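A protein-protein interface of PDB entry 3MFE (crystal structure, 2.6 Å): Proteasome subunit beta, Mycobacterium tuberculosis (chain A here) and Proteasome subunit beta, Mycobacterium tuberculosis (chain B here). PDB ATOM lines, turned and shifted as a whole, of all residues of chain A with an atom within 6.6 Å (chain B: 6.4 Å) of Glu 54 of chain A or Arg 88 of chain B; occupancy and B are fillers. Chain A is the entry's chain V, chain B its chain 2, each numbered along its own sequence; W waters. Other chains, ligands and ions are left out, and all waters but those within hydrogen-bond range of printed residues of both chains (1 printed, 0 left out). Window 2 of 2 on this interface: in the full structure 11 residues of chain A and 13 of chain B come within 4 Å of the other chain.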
ATOM      1  N   TYR A  35     -31.794  32.097  10.045  1.00  0.00           N
ATOM      2  CA  TYR A  35     -32.175  32.580   8.731  1.00  0.00           C
ATOM      3  C   TYR A  35     -33.632  32.357   8.375  1.00  0.00           C
ATOM      4  O   TYR A  35     -34.202  31.329   8.679  1.00  0.00           O
ATOM      5  CB  TYR A  35     -31.293  31.942   7.663  1.00  0.00           C
ATOM      6  CG  TYR A  35     -29.873  32.417   7.695  1.00  0.00           C
ATOM      7  CD1 TYR A  35     -29.513  33.617   7.108  1.00  0.00           C
ATOM      8  CD2 TYR A  35     -28.890  31.672   8.320  1.00  0.00           C
ATOM      9  CE1 TYR A  35     -28.224  34.060   7.147  1.00  0.00           C
ATOM     10  CE2 TYR A  35     -27.606  32.103   8.360  1.00  0.00           C
ATOM     11  CZ  TYR A  35     -27.273  33.295   7.769  1.00  0.00           C
ATOM     12  OH  TYR A  35     -25.977  33.722   7.801  1.00  0.00           O
ATOM     13  N   ALA A  50     -19.893  27.861  10.158  1.00  0.00           N
ATOM     14  CA  ALA A  50     -19.758  28.395   8.813  1.00  0.00           C
ATOM     15  C   ALA A  50     -20.875  27.852   7.919  1.00  0.00           C
ATOM     16  O   ALA A  50     -21.402  28.565   7.070  1.00  0.00           O
ATOM     17  CB  ALA A  50     -18.398  28.049   8.241  1.00  0.00           C
ATOM     18  N   VAL A  51     -21.220  26.584   8.123  1.00  0.00           N
ATOM     19  CA  VAL A  51     -22.242  25.884   7.338  1.00  0.00           C
ATOM     20  C   VAL A  51     -23.704  26.279   7.583  1.00  0.00           C
ATOM     21  O   VAL A  51     -24.583  25.869   6.832  1.00  0.00           O
ATOM     22  CB  VAL A  51     -22.124  24.357   7.480  1.00  0.00           C
ATOM     23  CG1 VAL A  51     -20.810  23.868   6.913  1.00  0.00           C
ATOM     24  CG2 VAL A  51     -22.279  23.948   8.926  1.00  0.00           C
ATOM     25  N   ALA A  52     -23.975  27.056   8.625  1.00  0.00           N
ATOM     26  CA  ALA A  52     -25.357  27.417   8.938  1.00  0.00           C
ATOM     27  C   ALA A  52     -26.029  28.148   7.782  1.00  0.00           C
ATOM     28  O   ALA A  52     -27.191  27.899   7.481  1.00  0.00           O
ATOM     29  CB  ALA A  52     -25.416  28.267  10.202  1.00  0.00           C
ATOM     30  N   VAL A  53     -25.301  29.043   7.133  1.00  0.00           N
ATOM     31  CA  VAL A  53     -25.832  29.776   5.993  1.00  0.00           C
ATOM     32  C   VAL A  53     -26.163  28.828   4.839  1.00  0.00           C
ATOM     33  O   VAL A  53     -27.133  29.023   4.121  1.00  0.00           O
ATOM     34  CB  VAL A  53     -24.854  30.854   5.511  1.00  0.00           C
ATOM     35  CG1 VAL A  53     -23.699  30.219   4.774  1.00  0.00           C
ATOM     36  CG2 VAL A  53     -25.564  31.863   4.631  1.00  0.00           C
ATOM     37  N   GLU A  54     -25.327  27.815   4.660  1.00  0.00           N
ATOM     38  CA  GLU A  54     -25.464  26.840   3.587  1.00  0.00           C
ATOM     39  C   GLU A  54     -26.672  25.903   3.715  1.00  0.00           C
ATOM     40  O   GLU A  54     -27.341  25.615   2.730  1.00  0.00           O
ATOM     41  CB  GLU A  54     -24.171  26.036   3.438  1.00  0.00           C
ATOM     42  CG  GLU A  54     -23.677  25.939   2.005  1.00  0.00           C
ATOM     43  CD  GLU A  54     -23.277  27.291   1.438  1.00  0.00           C
ATOM     44  OE1 GLU A  54     -22.471  27.992   2.080  1.00  0.00           O
ATOM     45  OE2 GLU A  54     -23.760  27.653   0.347  1.00  0.00           O
ATOM     46  N   PHE A  55     -26.927  25.415   4.926  1.00  0.00           N
ATOM     47  CA  PHE A  55     -28.059  24.523   5.196  1.00  0.00           C
ATOM     48  C   PHE A  55     -29.405  25.212   4.984  1.00  0.00           C
ATOM     49  O   PHE A  55     -30.321  24.660   4.391  1.00  0.00           O
ATOM     50  CB  PHE A  55     -27.962  24.032   6.640  1.00  0.00           C
ATOM     51  CG  PHE A  55     -28.595  22.694   6.879  1.00  0.00           C
ATOM     52  CD1 PHE A  55     -27.909  21.530   6.594  1.00  0.00           C
ATOM     53  CD2 PHE A  55     -29.863  22.600   7.414  1.00  0.00           C
ATOM     54  CE1 PHE A  55     -28.477  20.301   6.822  1.00  0.00           C
ATOM     55  CE2 PHE A  55     -30.437  21.373   7.644  1.00  0.00           C
ATOM     56  CZ  PHE A  55     -29.742  20.221   7.346  1.00  0.00           C
ATOM     57  N   ALA A  56     -29.482  26.437   5.479  1.00  0.00           N
ATOM     58  CA  ALA A  56     -30.601  27.351   5.320  1.00  0.00           C
ATOM     59  C   ALA A  56     -30.847  27.707   3.863  1.00  0.00           C
ATOM     60  O   ALA A  56     -31.992  27.715   3.402  1.00  0.00           O
ATOM     61  CB  ALA A  56     -30.380  28.603   6.120  1.00  0.00           C
ATOM     62  N   ARG A  57     -29.774  27.914   3.121  1.00  0.00           N
ATOM     63  CA  ARG A  57     -29.861  28.260   1.715  1.00  0.00           C
ATOM     64  C   ARG A  57     -30.475  27.123   0.901  1.00  0.00           C
ATOM     65  O   ARG A  57     -31.342  27.369   0.085  1.00  0.00           O
ATOM     66  CB  ARG A  57     -28.484  28.580   1.192  1.00  0.00           C
ATOM     67  CG  ARG A  57     -28.447  29.365  -0.073  1.00  0.00           C
ATOM     68  CD  ARG A  57     -27.036  29.873  -0.326  1.00  0.00           C
ATOM     69  NE  ARG A  57     -26.771  29.892  -1.754  1.00  0.00           N
ATOM     70  CZ  ARG A  57     -26.113  28.941  -2.402  1.00  0.00           C
ATOM     71  NH1 ARG A  57     -25.617  27.874  -1.752  1.00  0.00           N
ATOM     72  NH2 ARG A  57     -26.010  29.037  -3.713  1.00  0.00           N
ATOM     73  N   LEU A  58     -30.075  25.880   1.176  1.00  0.00           N
ATOM     74  CA  LEU A  58     -30.613  24.736   0.454  1.00  0.00           C
ATOM     75  C   LEU A  58     -32.085  24.439   0.820  1.00  0.00           C
ATOM     76  O   LEU A  58     -32.869  24.033  -0.036  1.00  0.00           O
ATOM     77  CB  LEU A  58     -29.753  23.509   0.718  1.00  0.00           C
ATOM     78  CG  LEU A  58     -30.114  22.152   0.097  1.00  0.00           C
ATOM     79  CD1 LEU A  58     -30.248  22.263  -1.394  1.00  0.00           C
ATOM     80  CD2 LEU A  58     -29.008  21.129   0.474  1.00  0.00           C
ATOM     81  N   TYR A  59     -32.416  24.585   2.093  1.00  0.00           N
ATOM     82  CA  TYR A  59     -33.763  24.377   2.594  1.00  0.00           C
ATOM     83  C   TYR A  59     -34.732  25.411   2.048  1.00  0.00           C
ATOM     84  O   TYR A  59     -35.867  25.104   1.736  1.00  0.00           O
ATOM     85  CB  TYR A  59     -33.754  24.363   4.118  1.00  0.00           C
ATOM     86  CG  TYR A  59     -35.088  24.112   4.770  1.00  0.00           C
ATOM     87  CD1 TYR A  59     -35.794  22.954   4.532  1.00  0.00           C
ATOM     88  CD2 TYR A  59     -35.626  25.028   5.647  1.00  0.00           C
ATOM     89  CE1 TYR A  59     -36.994  22.733   5.130  1.00  0.00           C
ATOM     90  CE2 TYR A  59     -36.820  24.809   6.247  1.00  0.00           C
ATOM     91  CZ  TYR A  59     -37.502  23.662   5.988  1.00  0.00           C
ATOM     92  OH  TYR A  59     -38.700  23.457   6.601  1.00  0.00           O
ATOM     93  N   MET A  86     -33.463  16.174   4.849  1.00  0.00           N
ATOM     94  CA  MET A  86     -32.169  16.861   4.676  1.00  0.00           C
ATOM     95  C   MET A  86     -31.173  16.467   5.791  1.00  0.00           C
ATOM     96  O   MET A  86     -30.008  16.154   5.536  1.00  0.00           O
ATOM     97  CB  MET A  86     -32.351  18.359   4.716  1.00  0.00           C
ATOM     98  CG  MET A  86     -32.229  19.010   3.396  1.00  0.00           C
ATOM     99  SD  MET A  86     -32.329  20.799   3.586  1.00  0.00           S
ATOM    100  CE  MET A  86     -30.728  21.075   4.161  1.00  0.00           C
ATOM    101  N   ASN B  81     -19.945  31.979  -3.462  1.00  0.00           N
ATOM    102  CA  ASN B  81     -20.528  30.649  -3.584  1.00  0.00           C
ATOM    103  C   ASN B  81     -19.679  29.691  -4.427  1.00  0.00           C
ATOM    104  O   ASN B  81     -19.432  28.536  -4.049  1.00  0.00           O
ATOM    105  CB  ASN B  81     -21.956  30.731  -4.106  1.00  0.00           C
ATOM    106  CG  ASN B  81     -22.734  29.474  -3.806  1.00  0.00           C
ATOM    107  OD1 ASN B  81     -22.736  28.980  -2.668  1.00  0.00           O
ATOM    108  ND2 ASN B  81     -23.342  28.902  -4.841  1.00  0.00           N
ATOM    109  N   LEU B  83     -16.447  29.786  -4.860  1.00  0.00           N
ATOM    110  CA  LEU B  83     -15.255  29.463  -4.117  1.00  0.00           C
ATOM    111  C   LEU B  83     -15.596  28.454  -3.038  1.00  0.00           C
ATOM    112  O   LEU B  83     -14.845  27.500  -2.840  1.00  0.00           O
ATOM    113  CB  LEU B  83     -14.599  30.716  -3.493  1.00  0.00           C
ATOM    114  CG  LEU B  83     -13.173  30.614  -2.876  1.00  0.00           C
ATOM    115  CD1 LEU B  83     -12.177  29.876  -3.799  1.00  0.00           C
ATOM    116  CD2 LEU B  83     -12.692  32.016  -2.590  1.00  0.00           C
ATOM    117  N   ALA B  84     -16.757  28.614  -2.404  1.00  0.00           N
ATOM    118  CA  ALA B  84     -17.191  27.711  -1.346  1.00  0.00           C
ATOM    119  C   ALA B  84     -17.379  26.311  -1.884  1.00  0.00           C
ATOM    120  O   ALA B  84     -16.977  25.335  -1.230  1.00  0.00           O
ATOM    121  CB  ALA B  84     -18.465  28.213  -0.691  1.00  0.00           C
ATOM    122  N   ILE B  85     -17.873  26.232  -3.125  1.00  0.00           N
ATOM    123  CA  ILE B  85     -18.105  24.945  -3.789  1.00  0.00           C
ATOM    124  C   ILE B  85     -16.793  24.245  -4.094  1.00  0.00           C
ATOM    125  O   ILE B  85     -16.648  23.053  -3.806  1.00  0.00           O
ATOM    126  CB  ILE B  85     -19.058  25.089  -5.037  1.00  0.00           C
ATOM    127  CG1 ILE B  85     -20.501  25.286  -4.539  1.00  0.00           C
ATOM    128  CG2 ILE B  85     -19.015  23.843  -5.931  1.00  0.00           C
ATOM    129  CD1 ILE B  85     -21.446  25.889  -5.542  1.00  0.00           C
ATOM    130  N   MET B  86     -15.816  25.021  -4.562  1.00  0.00           N
ATOM    131  CA  MET B  86     -14.476  24.516  -4.866  1.00  0.00           C
ATOM    132  C   MET B  86     -13.796  23.938  -3.623  1.00  0.00           C
ATOM    133  O   MET B  86     -13.222  22.868  -3.685  1.00  0.00           O
ATOM    134  CB  MET B  86     -13.612  25.637  -5.405  1.00  0.00           C
ATOM    135  CG  MET B  86     -13.327  25.524  -6.864  1.00  0.00           C
ATOM    136  SD  MET B  86     -12.189  26.796  -7.384  1.00  0.00           S
ATOM    137  CE  MET B  86     -10.751  26.108  -6.802  1.00  0.00           C
ATOM    138  N   VAL B  87     -13.942  24.619  -2.491  1.00  0.00           N
ATOM    139  CA  VAL B  87     -13.339  24.189  -1.236  1.00  0.00           C
ATOM    140  C   VAL B  87     -14.028  22.945  -0.702  1.00  0.00           C
ATOM    141  O   VAL B  87     -13.344  22.032  -0.237  1.00  0.00           O
ATOM    142  CB  VAL B  87     -13.359  25.324  -0.170  1.00  0.00           C
ATOM    143  CG1 VAL B  87     -12.698  24.892   1.147  1.00  0.00           C
ATOM    144  CG2 VAL B  87     -12.638  26.526  -0.712  1.00  0.00           C
ATOM    145  N   ARG B  88     -15.358  22.889  -0.831  1.00  0.00           N
ATOM    146  CA  ARG B  88     -16.175  21.762  -0.363  1.00  0.00           C
ATOM    147  C   ARG B  88     -15.859  20.521  -1.178  1.00  0.00           C
ATOM    148  O   ARG B  88     -15.843  19.410  -0.644  1.00  0.00           O
ATOM    149  CB  ARG B  88     -17.662  22.091  -0.472  1.00  0.00           C
ATOM    150  CG  ARG B  88     -18.607  21.276   0.426  1.00  0.00           C
ATOM    151  CD  ARG B  88     -20.001  21.921   0.470  1.00  0.00           C
ATOM    152  NE  ARG B  88     -20.028  23.226   1.167  1.00  0.00           N
ATOM    153  CZ  ARG B  88     -20.553  24.359   0.683  1.00  0.00           C
ATOM    154  NH1 ARG B  88     -21.121  24.397  -0.524  1.00  0.00           N
ATOM    155  NH2 ARG B  88     -20.496  25.470   1.416  1.00  0.00           N
ATOM    156  N   GLY B  89     -15.521  20.730  -2.451  1.00  0.00           N
ATOM    157  CA  GLY B  89     -15.171  19.631  -3.348  1.00  0.00           C
ATOM    158  C   GLY B  89     -13.791  19.030  -3.095  1.00  0.00           C
ATOM    159  O   GLY B  89     -13.407  18.046  -3.719  1.00  0.00           O
ATOM    160  N   ASN B  90     -13.072  19.622  -2.147  1.00  0.00           N
ATOM    161  CA  ASN B  90     -11.742  19.197  -1.762  1.00  0.00           C
ATOM    162  C   ASN B  90     -11.758  18.730  -0.286  1.00  0.00           C
ATOM    163  O   ASN B  90     -10.712  18.653   0.362  1.00  0.00           O
ATOM    164  CB  ASN B  90     -10.764  20.367  -1.999  1.00  0.00           C
ATOM    165  CG  ASN B  90      -9.298  19.945  -1.941  1.00  0.00           C
ATOM    166  OD1 ASN B  90      -8.549  20.378  -1.058  1.00  0.00           O
ATOM    167  ND2 ASN B  90      -8.892  19.085  -2.864  1.00  0.00           N
ATOM    168  N   LEU B  91     -12.943  18.382   0.225  1.00  0.00           N
ATOM    169  CA  LEU B  91     -13.085  17.901   1.611  1.00  0.00           C
ATOM    170  C   LEU B  91     -12.590  16.453   1.755  1.00  0.00           C
ATOM    171  O   LEU B  91     -11.957  16.119   2.763  1.00  0.00           O
ATOM    172  CB  LEU B  91     -14.540  18.022   2.115  1.00  0.00           C
ATOM    173  CG  LEU B  91     -14.959  17.556   3.533  1.00  0.00           C
ATOM    174  CD1 LEU B  91     -14.273  18.387   4.631  1.00  0.00           C
ATOM    175  CD2 LEU B  91     -16.478  17.618   3.674  1.00  0.00           C
ATOM    176  N   ALA B  92     -12.854  15.624   0.731  1.00  0.00           N
ATOM    177  CA  ALA B  92     -12.442  14.206   0.692  1.00  0.00           C
ATOM    178  C   ALA B  92     -10.902  14.052   0.712  1.00  0.00           C
ATOM    179  O   ALA B  92     -10.361  13.156   1.384  1.00  0.00           O
ATOM    180  CB  ALA B  92     -13.039  13.513  -0.544  1.00  0.00           C
ATOM    181  N   ALA B 125     -12.526  24.384   7.057  1.00  0.00           N
ATOM    182  CA  ALA B 125     -12.301  23.029   6.533  1.00  0.00           C
ATOM    183  C   ALA B 125     -13.457  22.460   5.681  1.00  0.00           C
ATOM    184  O   ALA B 125     -13.251  22.033   4.533  1.00  0.00           O
ATOM    185  CB  ALA B 125     -11.962  22.065   7.713  1.00  0.00           C
ATOM    186  N   ALA B 126     -14.672  22.588   6.223  1.00  0.00           N
ATOM    187  CA  ALA B 126     -15.915  22.097   5.604  1.00  0.00           C
ATOM    188  C   ALA B 126     -16.385  22.829   4.331  1.00  0.00           C
ATOM    189  O   ALA B 126     -17.263  22.331   3.617  1.00  0.00           O
ATOM    190  CB  ALA B 126     -17.053  22.074   6.671  1.00  0.00           C
ATOM    191  N   GLY B 127     -15.783  23.989   4.052  1.00  0.00           N
ATOM    192  CA  GLY B 127     -16.146  24.787   2.890  1.00  0.00           C
ATOM    193  C   GLY B 127     -17.154  25.849   3.288  1.00  0.00           C
ATOM    194  O   GLY B 127     -17.928  26.356   2.465  1.00  0.00           O
ATOM    195  N   GLY B 128     -17.160  26.156   4.581  1.00  0.00           N
ATOM    196  CA  GLY B 128     -18.062  27.153   5.113  1.00  0.00           C
ATOM    197  C   GLY B 128     -17.420  28.513   5.053  1.00  0.00           C
ATOM    198  O   GLY B 128     -16.235  28.660   5.393  1.00  0.00           O
ATOM    199  N   TRP B 129     -18.221  29.506   4.668  1.00  0.00           N
ATOM    200  CA  TRP B 129     -17.742  30.867   4.536  1.00  0.00           C
ATOM    201  C   TRP B 129     -18.266  31.838   5.574  1.00  0.00           C
ATOM    202  O   TRP B 129     -19.338  31.624   6.129  1.00  0.00           O
ATOM    203  CB  TRP B 129     -18.046  31.379   3.130  1.00  0.00           C
ATOM    204  CG  TRP B 129     -19.463  31.284   2.732  1.00  0.00           C
ATOM    205  CD1 TRP B 129     -20.114  30.177   2.268  1.00  0.00           C
ATOM    206  CD2 TRP B 129     -20.431  32.328   2.811  1.00  0.00           C
ATOM    207  NE1 TRP B 129     -21.429  30.469   2.061  1.00  0.00           N
ATOM    208  CE2 TRP B 129     -21.659  31.781   2.386  1.00  0.00           C
ATOM    209  CE3 TRP B 129     -20.385  33.674   3.223  1.00  0.00           C
ATOM    210  CZ2 TRP B 129     -22.863  32.543   2.359  1.00  0.00           C
ATOM    211  CZ3 TRP B 129     -21.582  34.439   3.205  1.00  0.00           C
ATOM    212  CH2 TRP B 129     -22.805  33.865   2.775  1.00  0.00           C
HETATM  213  O   HOH W   1     -22.135  26.477  -1.915  1.00  0.00           O
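The side-chain carboxylate (OE2) of Glu 54 of chain A sits close to the side-chain amide oxygen (OD1) of Asn 81 of chain B, 3.4 Å away. ND2 of Asn 81 of chain B sits close to NH2 of Arg 57 of chain A. OE1 of Glu 54 of chain A lies within salt-bridge range of NH2 of Arg 88 of chain B, at 3.3 Å. NE1 of Trp 129 of chain B lies within hydrogen-bond range of OE1 of Glu 54 of chain A (2.7 Å).
The backbone carbonyl oxygen of Gly 127 of chain B lies within hydrogen-bond range of the guanidinium group of Arg 88 of chain B (2.9 Å). The side-chain carboxylate of Glu 54 of chain A is in salt-bridge range of the guanidinium group of Arg 57 of chain A (2.8 Å).
Among the printed residues, pairs that only touch across the chains: Ala 50 of chain A with Gly 128 of chain B, Ala 50 of chain A with Trp 129 of chain B and Val 53 of chain A with Trp 129 of chain B.
Glu 54 of chain A touches just these residues of chain B: Asn 81, Arg 88 and Trp 129. Arg 88 of chain B touches just one residue of chain A: Glu 54. Of the printed residues of chain B, Val 53 of chain A touches Trp 129. Of the printed residues of chain B, Arg 57 of chain A touches Asn 81 (2.9 Å). Printed residues of chain A within 4 Å of Asn 81 of chain B: Glu 54 and Arg 57. Of the printed residues of chain B, Ala 50 of chain A touches Gly 128 and Trp 129. The nearest residue of chain B that does not touch Glu 54 of chain A is Gly 127 of chain B (4.8 Å).
Printed residues of chain B that touch a printed residue of chain A: Asn 81, Arg 88, Gly 128 and Trp 129. Hydrophobic or aromatic side chains of chain B within 4 Å of the printed part of chain A: Trp 129. Along chain B the printed residues that touch a printed residue of chain A span positions 81 to 129. Printed residues of chain A that touch a printed residue of chain B: Ala 50, Val 53, Glu 54 and Arg 57. Hydrophobic or aromatic side chains of chain A that line the printed part of chain B: Ala 50 and Val 53. Among the printed residues, Asp or Glu carboxylates within 4 Å of a Lys or Arg side-chain nitrogen of the other chain: Glu 54 of chain A with Arg 88 of chain B.
Water W1 lies within hydrogen-bond range of the side-chain amide oxygen (OD1) of Asn 81 of chain B, the guanidinium group (NH1) of Arg 88 of chain B and the side-chain carboxylate (OE2) of Glu 54 of chain A.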
